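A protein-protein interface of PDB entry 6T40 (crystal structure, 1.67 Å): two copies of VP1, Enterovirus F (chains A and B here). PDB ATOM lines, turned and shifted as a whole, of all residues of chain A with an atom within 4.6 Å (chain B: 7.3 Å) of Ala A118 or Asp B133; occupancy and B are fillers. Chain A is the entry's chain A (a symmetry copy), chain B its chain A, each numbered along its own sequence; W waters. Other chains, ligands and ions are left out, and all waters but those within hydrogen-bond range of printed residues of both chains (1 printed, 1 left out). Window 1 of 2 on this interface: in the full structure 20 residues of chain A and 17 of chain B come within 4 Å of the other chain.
OD2 of Asp B133 sits close to OE1 of Gln A119, 3.0 Å away. The guanidinium group (NE) of Arg A227 is in salt-bridge range of the side-chain carboxylate (OE2) of Glu B219, 3.1 Å away.
Of the printed residues of chain B, Ala A118 touches Asp B133. Printed residues of chain A within 4 Å of Glu B219: Gln A119 and Arg A227. Of the printed residues of chain B, Gln A119 touches Asp B133 and Glu B219. Of the printed residues of chain B, Arg A227 touches Glu B219. Ile B163 touches none of the printed residues of chain A. The nearest printed residue of chain B that does not touch Arg A227 is Cys B218 (6.1 Å).
OD1 of Asp B133 is in hydrogen-bond range of ND2 of Asn B165 (2.9 Å). O of Asp B133 is in hydrogen-bond range of N of Cys B218, at 3.1 Å. OG1 of Thr B217 sits at hydrogen-bond distance from O of Glu B219 (2.7 Å). The backbone carbonyl oxygen (O) of Gln A119 lies within hydrogen-bond range of the backbone NH (N) of Arg A227 (2.7 Å).
Water W1 lies within hydrogen-bond range of OE1 of Glu B219 (2.8 Å) and NE of Arg A227 (3.4 Å).
Asp B133 touches Ala A118. NE2 of Gln A119 touches CG of Glu B219, at 3.6 Å.
3 positions are printed for both chains.
Of the 18 printed residues of chain B, 2 touch a printed residue of chain A. Along chain B the printed residues that touch a printed residue of chain A span positions 133 to 219. Among the printed residues, 4 pairs touch across the chains.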
ATOM      1  N   ILE A 116     -22.358 -12.897   6.985  1.00  0.00           N
ATOM      2  CA  ILE A 116     -21.650 -13.626   8.027  1.00  0.00           C
ATOM      3  C   ILE A 116     -20.834 -14.785   7.467  1.00  0.00           C
ATOM      4  O   ILE A 116     -21.366 -15.663   6.791  1.00  0.00           O
ATOM      5  CB  ILE A 116     -22.656 -14.149   9.076  1.00  0.00           C
ATOM      6  CG1 ILE A 116     -23.408 -12.958   9.684  1.00  0.00           C
ATOM      7  CG2 ILE A 116     -21.936 -14.948  10.158  1.00  0.00           C
ATOM      8  CD1 ILE A 116     -24.521 -13.343  10.628  1.00  0.00           C
ATOM      9  N   VAL A 117     -19.535 -14.767   7.749  1.00  0.00           N
ATOM     10  CA  VAL A 117     -18.622 -15.810   7.294  1.00  0.00           C
ATOM     11  C   VAL A 117     -18.114 -16.531   8.538  1.00  0.00           C
ATOM     12  O   VAL A 117     -17.499 -15.918   9.411  1.00  0.00           O
ATOM     13  CB  VAL A 117     -17.419 -15.208   6.533  1.00  0.00           C
ATOM     14  CG1 VAL A 117     -16.521 -16.323   6.011  1.00  0.00           C
ATOM     15  CG2 VAL A 117     -17.914 -14.336   5.381  1.00  0.00           C
ATOM     16  N   ALA A 118     -18.365 -17.832   8.617  1.00  0.00           N
ATOM     17  CA  ALA A 118     -17.948 -18.598   9.782  1.00  0.00           C
ATOM     18  C   ALA A 118     -17.251 -19.906   9.441  1.00  0.00           C
ATOM     19  O   ALA A 118     -17.530 -20.528   8.417  1.00  0.00           O
ATOM     20  CB  ALA A 118     -19.161 -18.882  10.662  1.00  0.00           C
ATOM     21  N   GLN A 119     -16.331 -20.313  10.306  1.00  0.00           N
ATOM     22  CA  GLN A 119     -15.630 -21.573  10.121  1.00  0.00           C
ATOM     23  C   GLN A 119     -15.187 -22.087  11.480  1.00  0.00           C
ATOM     24  O   GLN A 119     -15.173 -21.348  12.461  1.00  0.00           O
ATOM     25  CB  GLN A 119     -14.425 -21.423   9.180  1.00  0.00           C
ATOM     26  CG  GLN A 119     -13.357 -20.444   9.613  1.00  0.00           C
ATOM     27  CD  GLN A 119     -13.690 -19.012   9.250  1.00  0.00           C
ATOM     28  OE1 GLN A 119     -13.972 -18.698   8.092  1.00  0.00           O
ATOM     29  NE2 GLN A 119     -13.645 -18.132  10.238  1.00  0.00           N
ATOM     30  N   TYR A 134     -24.807 -23.324  12.649  1.00  0.00           N
ATOM     31  CA  TYR A 134     -24.664 -22.263  13.632  1.00  0.00           C
ATOM     32  C   TYR A 134     -25.899 -21.376  13.578  1.00  0.00           C
ATOM     33  O   TYR A 134     -26.610 -21.339  12.572  1.00  0.00           O
ATOM     34  CB  TYR A 134     -23.391 -21.448  13.369  1.00  0.00           C
ATOM     35  CG  TYR A 134     -23.368 -20.700  12.055  1.00  0.00           C
ATOM     36  CD1 TYR A 134     -23.919 -19.423  11.946  1.00  0.00           C
ATOM     37  CD2 TYR A 134     -22.789 -21.267  10.916  1.00  0.00           C
ATOM     38  CE1 TYR A 134     -23.890 -18.725  10.739  1.00  0.00           C
ATOM     39  CE2 TYR A 134     -22.758 -20.578   9.701  1.00  0.00           C
ATOM     40  CZ  TYR A 134     -23.311 -19.307   9.623  1.00  0.00           C
ATOM     41  OH  TYR A 134     -23.286 -18.619   8.429  1.00  0.00           O
ATOM     42  N   THR A 166     -21.401 -23.863   8.227  1.00  0.00           N
ATOM     43  CA  THR A 166     -20.085 -23.435   7.765  1.00  0.00           C
ATOM     44  C   THR A 166     -19.788 -24.061   6.404  1.00  0.00           C
ATOM     45  O   THR A 166     -18.847 -23.662   5.719  1.00  0.00           O
ATOM     46  CB  THR A 166     -18.981 -23.833   8.766  1.00  0.00           C
ATOM     47  OG1 THR A 166     -19.045 -25.239   9.020  1.00  0.00           O
ATOM     48  CG2 THR A 166     -19.155 -23.073  10.077  1.00  0.00           C
ATOM     49  N   LEU A 226     -16.193 -21.952  17.081  1.00  0.00           N
ATOM     50  CA  LEU A 226     -16.697 -21.339  15.859  1.00  0.00           C
ATOM     51  C   LEU A 226     -16.092 -19.943  15.732  1.00  0.00           C
ATOM     52  O   LEU A 226     -16.199 -19.125  16.646  1.00  0.00           O
ATOM     53  CB  LEU A 226     -18.225 -21.229  15.897  1.00  0.00           C
ATOM     54  CG  LEU A 226     -18.867 -20.719  14.603  1.00  0.00           C
ATOM     55  CD1 LEU A 226     -18.787 -21.804  13.533  1.00  0.00           C
ATOM     56  CD2 LEU A 226     -20.317 -20.341  14.858  1.00  0.00           C
ATOM     57  N   ARG A 227     -15.443 -19.690  14.601  1.00  0.00           N
ATOM     58  CA  ARG A 227     -14.832 -18.394  14.316  1.00  0.00           C
ATOM     59  C   ARG A 227     -15.840 -17.664  13.434  1.00  0.00           C
ATOM     60  O   ARG A 227     -16.317 -18.220  12.444  1.00  0.00           O
ATOM     61  CB  ARG A 227     -13.515 -18.593  13.565  1.00  0.00           C
ATOM     62  CG  ARG A 227     -12.766 -17.316  13.230  1.00  0.00           C
ATOM     63  CD  ARG A 227     -12.304 -16.597  14.482  1.00  0.00           C
ATOM     64  NE  ARG A 227     -11.344 -15.540  14.177  1.00  0.00           N
ATOM     65  CZ  ARG A 227     -10.878 -14.677  15.074  1.00  0.00           C
ATOM     66  NH1 ARG A 227     -11.284 -14.745  16.336  1.00  0.00           N
ATOM     67  NH2 ARG A 227     -10.000 -13.752  14.711  1.00  0.00           N
ATOM     68  N   VAL A 228     -16.164 -16.428  13.789  1.00  0.00           N
ATOM     69  CA  VAL A 228     -17.153 -15.670  13.033  1.00  0.00           C
ATOM     70  C   VAL A 228     -16.715 -14.265  12.649  1.00  0.00           C
ATOM     71  O   VAL A 228     -16.112 -13.547  13.446  1.00  0.00           O
ATOM     72  CB  VAL A 228     -18.471 -15.539  13.843  1.00  0.00           C
ATOM     73  CG1 VAL A 228     -19.513 -14.774  13.035  1.00  0.00           C
ATOM     74  CG2 VAL A 228     -18.990 -16.919  14.231  1.00  0.00           C
ATOM     75  N   PHE B 130      -9.615 -30.515   1.131  1.00  0.00           N
ATOM     76  CA  PHE B 130      -9.821 -29.702   2.319  1.00  0.00           C
ATOM     77  C   PHE B 130     -10.484 -28.390   1.922  1.00  0.00           C
ATOM     78  O   PHE B 130      -9.907 -27.596   1.182  1.00  0.00           O
ATOM     79  CB  PHE B 130      -8.453 -29.450   2.972  1.00  0.00           C
ATOM     80  CG  PHE B 130      -8.521 -28.822   4.336  1.00  0.00           C
ATOM     81  CD1 PHE B 130      -8.795 -27.466   4.484  1.00  0.00           C
ATOM     82  CD2 PHE B 130      -8.285 -29.587   5.474  1.00  0.00           C
ATOM     83  CE1 PHE B 130      -8.834 -26.879   5.752  1.00  0.00           C
ATOM     84  CE2 PHE B 130      -8.321 -29.012   6.745  1.00  0.00           C
ATOM     85  CZ  PHE B 130      -8.594 -27.655   6.884  1.00  0.00           C
ATOM     86  N   ASN B 131     -11.702 -28.175   2.405  1.00  0.00           N
ATOM     87  CA  ASN B 131     -12.429 -26.951   2.091  1.00  0.00           C
ATOM     88  C   ASN B 131     -12.023 -25.851   3.053  1.00  0.00           C
ATOM     89  O   ASN B 131     -12.117 -26.013   4.268  1.00  0.00           O
ATOM     90  CB  ASN B 131     -13.940 -27.176   2.190  1.00  0.00           C
ATOM     91  CG  ASN B 131     -14.440 -28.208   1.201  1.00  0.00           C
ATOM     92  OD1 ASN B 131     -13.830 -28.429   0.155  1.00  0.00           O
ATOM     93  ND2 ASN B 131     -15.565 -28.835   1.521  1.00  0.00           N
ATOM     94  N   VAL B 132     -11.569 -24.729   2.509  1.00  0.00           N
ATOM     95  CA  VAL B 132     -11.158 -23.611   3.343  1.00  0.00           C
ATOM     96  C   VAL B 132     -11.589 -22.299   2.704  1.00  0.00           C
ATOM     97  O   VAL B 132     -11.614 -22.177   1.477  1.00  0.00           O
ATOM     98  CB  VAL B 132      -9.619 -23.603   3.548  1.00  0.00           C
ATOM     99  CG1 VAL B 132      -8.909 -23.369   2.217  1.00  0.00           C
ATOM    100  CG2 VAL B 132      -9.230 -22.532   4.559  1.00  0.00           C
ATOM    101  N   ASP B 133     -11.947 -21.328   3.537  1.00  0.00           N
ATOM    102  CA  ASP B 133     -12.352 -20.018   3.043  1.00  0.00           C
ATOM    103  C   ASP B 133     -11.100 -19.214   2.725  1.00  0.00           C
ATOM    104  O   ASP B 133     -10.133 -19.228   3.487  1.00  0.00           O
ATOM    105  CB  ASP B 133     -13.168 -19.266   4.098  1.00  0.00           C
ATOM    106  CG  ASP B 133     -14.492 -19.939   4.402  1.00  0.00           C
ATOM    107  OD1 ASP B 133     -15.286 -20.149   3.460  1.00  0.00           O
ATOM    108  OD2 ASP B 133     -14.743 -20.251   5.586  1.00  0.00           O
ATOM    109  N   TYR B 134     -11.113 -18.521   1.593  1.00  0.00           N
ATOM    110  CA  TYR B 134      -9.978 -17.699   1.207  1.00  0.00           C
ATOM    111  C   TYR B 134     -10.486 -16.327   0.789  1.00  0.00           C
ATOM    112  O   TYR B 134     -11.652 -16.168   0.425  1.00  0.00           O
ATOM    113  CB  TYR B 134      -9.189 -18.361   0.070  1.00  0.00           C
ATOM    114  CG  TYR B 134      -9.949 -18.523  -1.228  1.00  0.00           C
ATOM    115  CD1 TYR B 134      -9.982 -17.498  -2.172  1.00  0.00           C
ATOM    116  CD2 TYR B 134     -10.631 -19.708  -1.517  1.00  0.00           C
ATOM    117  CE1 TYR B 134     -10.672 -17.646  -3.375  1.00  0.00           C
ATOM    118  CE2 TYR B 134     -11.328 -19.866  -2.717  1.00  0.00           C
ATOM    119  CZ  TYR B 134     -11.342 -18.830  -3.641  1.00  0.00           C
ATOM    120  OH  TYR B 134     -12.028 -18.976  -4.827  1.00  0.00           O
ATOM    121  N   GLN B 135      -9.610 -15.335   0.863  1.00  0.00           N
ATOM    122  CA  GLN B 135      -9.976 -13.977   0.506  1.00  0.00           C
ATOM    123  C   GLN B 135      -8.978 -13.402  -0.483  1.00  0.00           C
ATOM    124  O   GLN B 135      -7.766 -13.519  -0.296  1.00  0.00           O
ATOM    125  CB  GLN B 135     -10.015 -13.098   1.760  1.00  0.00           C
ATOM    126  CG  GLN B 135     -10.381 -11.638   1.501  1.00  0.00           C
ATOM    127  CD  GLN B 135     -10.422 -10.819   2.780  1.00  0.00           C
ATOM    128  OE1 GLN B 135     -10.218 -11.347   3.874  1.00  0.00           O
ATOM    129  NE2 GLN B 135     -10.689  -9.524   2.650  1.00  0.00           N
ATOM    130  N   ILE B 163     -14.504 -13.204  -1.194  1.00  0.00           N
ATOM    131  CA  ILE B 163     -14.272 -14.289  -0.259  1.00  0.00           C
ATOM    132  C   ILE B 163     -15.029 -15.504  -0.762  1.00  0.00           C
ATOM    133  O   ILE B 163     -16.231 -15.435  -1.017  1.00  0.00           O
ATOM    134  CB  ILE B 163     -14.786 -13.926   1.155  1.00  0.00           C
ATOM    135  CG1 ILE B 163     -13.909 -12.825   1.756  1.00  0.00           C
ATOM    136  CG2 ILE B 163     -14.797 -15.163   2.045  1.00  0.00           C
ATOM    137  CD1 ILE B 163     -14.431 -12.278   3.069  1.00  0.00           C
ATOM    138  N   SER B 164     -14.322 -16.610  -0.936  1.00  0.00           N
ATOM    139  CA  SER B 164     -14.972 -17.827  -1.384  1.00  0.00           C
ATOM    140  C   SER B 164     -14.374 -19.010  -0.640  1.00  0.00           C
ATOM    141  O   SER B 164     -13.681 -18.831   0.362  1.00  0.00           O
ATOM    142  CB  SER B 164     -14.829 -18.006  -2.896  1.00  0.00           C
ATOM    143  OG  SER B 164     -15.741 -18.993  -3.353  1.00  0.00           O
ATOM    144  N   ASN B 165     -14.629 -20.212  -1.138  1.00  0.00           N
ATOM    145  CA  ASN B 165     -14.153 -21.422  -0.482  1.00  0.00           C
ATOM    146  C   ASN B 165     -13.640 -22.405  -1.528  1.00  0.00           C
ATOM    147  O   ASN B 165     -14.174 -22.474  -2.636  1.00  0.00           O
ATOM    148  CB  ASN B 165     -15.321 -22.026   0.310  1.00  0.00           C
ATOM    149  CG  ASN B 165     -14.894 -23.129   1.256  1.00  0.00           C
ATOM    150  OD1 ASN B 165     -14.499 -24.213   0.830  1.00  0.00           O
ATOM    151  ND2 ASN B 165     -14.978 -22.857   2.555  1.00  0.00           N
ATOM    152  N   THR B 166     -12.600 -23.159  -1.185  1.00  0.00           N
ATOM    153  CA  THR B 166     -12.050 -24.131  -2.123  1.00  0.00           C
ATOM    154  C   THR B 166     -13.083 -25.219  -2.406  1.00  0.00           C
ATOM    155  O   THR B 166     -12.930 -26.007  -3.338  1.00  0.00           O
ATOM    156  CB  THR B 166     -10.760 -24.776  -1.574  1.00  0.00           C
ATOM    157  OG1 THR B 166     -11.016 -25.340  -0.284  1.00  0.00           O
ATOM    158  CG2 THR B 166      -9.653 -23.734  -1.460  1.00  0.00           C
ATOM    159  N   GLY B 167     -14.140 -25.247  -1.598  1.00  0.00           N
ATOM    160  CA  GLY B 167     -15.195 -26.230  -1.781  1.00  0.00           C
ATOM    161  C   GLY B 167     -16.307 -25.723  -2.685  1.00  0.00           C
ATOM    162  O   GLY B 167     -17.229 -26.461  -3.024  1.00  0.00           O
ATOM    163  N   LEU B 168     -16.227 -24.453  -3.070  1.00  0.00           N
ATOM    164  CA  LEU B 168     -17.223 -23.849  -3.953  1.00  0.00           C
ATOM    165  C   LEU B 168     -16.644 -23.755  -5.358  1.00  0.00           C
ATOM    166  O   LEU B 168     -15.456 -24.001  -5.562  1.00  0.00           O
ATOM    167  CB  LEU B 168     -17.578 -22.440  -3.470  1.00  0.00           C
ATOM    168  CG  LEU B 168     -18.466 -22.303  -2.233  1.00  0.00           C
ATOM    169  CD1 LEU B 168     -18.491 -20.845  -1.773  1.00  0.00           C
ATOM    170  CD2 LEU B 168     -19.872 -22.790  -2.566  1.00  0.00           C
ATOM    171  N   ARG B 216      -5.212 -14.630   0.971  1.00  0.00           N
ATOM    172  CA  ARG B 216      -4.984 -15.267   2.262  1.00  0.00           C
ATOM    173  C   ARG B 216      -6.094 -16.268   2.521  1.00  0.00           C
ATOM    174  O   ARG B 216      -7.105 -16.286   1.816  1.00  0.00           O
ATOM    175  CB  ARG B 216      -5.031 -14.240   3.401  1.00  0.00           C
ATOM    176  CG  ARG B 216      -6.449 -13.719   3.691  1.00  0.00           C
ATOM    177  CD  ARG B 216      -6.595 -13.133   5.096  1.00  0.00           C
ATOM    178  NE  ARG B 216      -7.960 -12.662   5.344  1.00  0.00           N
ATOM    179  CZ  ARG B 216      -8.403 -12.210   6.514  1.00  0.00           C
ATOM    180  NH1 ARG B 216      -7.595 -12.160   7.566  1.00  0.00           N
ATOM    181  NH2 ARG B 216      -9.663 -11.805   6.636  1.00  0.00           N
ATOM    182  N   THR B 217      -5.887 -17.122   3.516  1.00  0.00           N
ATOM    183  CA  THR B 217      -6.937 -18.031   3.937  1.00  0.00           C
ATOM    184  C   THR B 217      -7.460 -17.211   5.116  1.00  0.00           C
ATOM    185  O   THR B 217      -6.673 -16.567   5.816  1.00  0.00           O
ATOM    186  CB  THR B 217      -6.394 -19.393   4.425  1.00  0.00           C
ATOM    187  OG1 THR B 217      -5.322 -19.186   5.353  1.00  0.00           O
ATOM    188  CG2 THR B 217      -5.905 -20.220   3.243  1.00  0.00           C
ATOM    189  N   CYS B 218      -8.772 -17.193   5.322  1.00  0.00           N
ATOM    190  CA  CYS B 218      -9.348 -16.406   6.410  1.00  0.00           C
ATOM    191  C   CYS B 218      -8.810 -16.802   7.782  1.00  0.00           C
ATOM    192  O   CYS B 218      -8.667 -15.957   8.666  1.00  0.00           O
ATOM    193  CB  CYS B 218     -10.872 -16.515   6.371  1.00  0.00           C
ATOM    194  SG  CYS B 218     -11.557 -15.834   4.833  1.00  0.00           S
ATOM    195  N   GLU B 219      -8.521 -18.086   7.956  1.00  0.00           N
ATOM    196  CA  GLU B 219      -7.957 -18.586   9.205  1.00  0.00           C
ATOM    197  C   GLU B 219      -6.722 -19.411   8.848  1.00  0.00           C
ATOM    198  O   GLU B 219      -6.553 -19.809   7.695  1.00  0.00           O
ATOM    199  CB  GLU B 219      -8.985 -19.430   9.968  1.00  0.00           C
ATOM    200  CG  GLU B 219     -10.140 -18.614  10.555  1.00  0.00           C
ATOM    201  CD  GLU B 219      -9.673 -17.549  11.541  1.00  0.00           C
ATOM    202  OE1 GLU B 219      -8.863 -17.874  12.435  1.00  0.00           O
ATOM    203  OE2 GLU B 219     -10.121 -16.387  11.434  1.00  0.00           O
ATOM    204  N   LEU B 221      -4.095 -22.309   8.191  1.00  0.00           N
ATOM    205  CA  LEU B 221      -4.060 -23.717   7.815  1.00  0.00           C
ATOM    206  C   LEU B 221      -2.977 -24.355   8.679  1.00  0.00           C
ATOM    207  O   LEU B 221      -2.004 -23.698   9.049  1.00  0.00           O
ATOM    208  CB  LEU B 221      -3.689 -23.878   6.340  1.00  0.00           C
ATOM    209  CG  LEU B 221      -4.788 -23.585   5.319  1.00  0.00           C
ATOM    210  CD1 LEU B 221      -4.194 -23.555   3.916  1.00  0.00           C
ATOM    211  CD2 LEU B 221      -5.870 -24.651   5.427  1.00  0.00           C
ATOM    212  N   LEU B 226      -2.301 -22.629   0.495  1.00  0.00           N
ATOM    213  CA  LEU B 226      -3.340 -22.421  -0.504  1.00  0.00           C
ATOM    214  C   LEU B 226      -2.673 -22.224  -1.864  1.00  0.00           C
ATOM    215  O   LEU B 226      -1.808 -21.362  -2.023  1.00  0.00           O
ATOM    216  CB  LEU B 226      -4.178 -21.184  -0.167  1.00  0.00           C
ATOM    217  CG  LEU B 226      -5.384 -20.951  -1.083  1.00  0.00           C
ATOM    218  CD1 LEU B 226      -6.460 -21.990  -0.783  1.00  0.00           C
ATOM    219  CD2 LEU B 226      -5.935 -19.551  -0.870  1.00  0.00           C
HETATM  220  O   HOH W   1      -8.660 -17.451  15.166  1.00  0.00           O
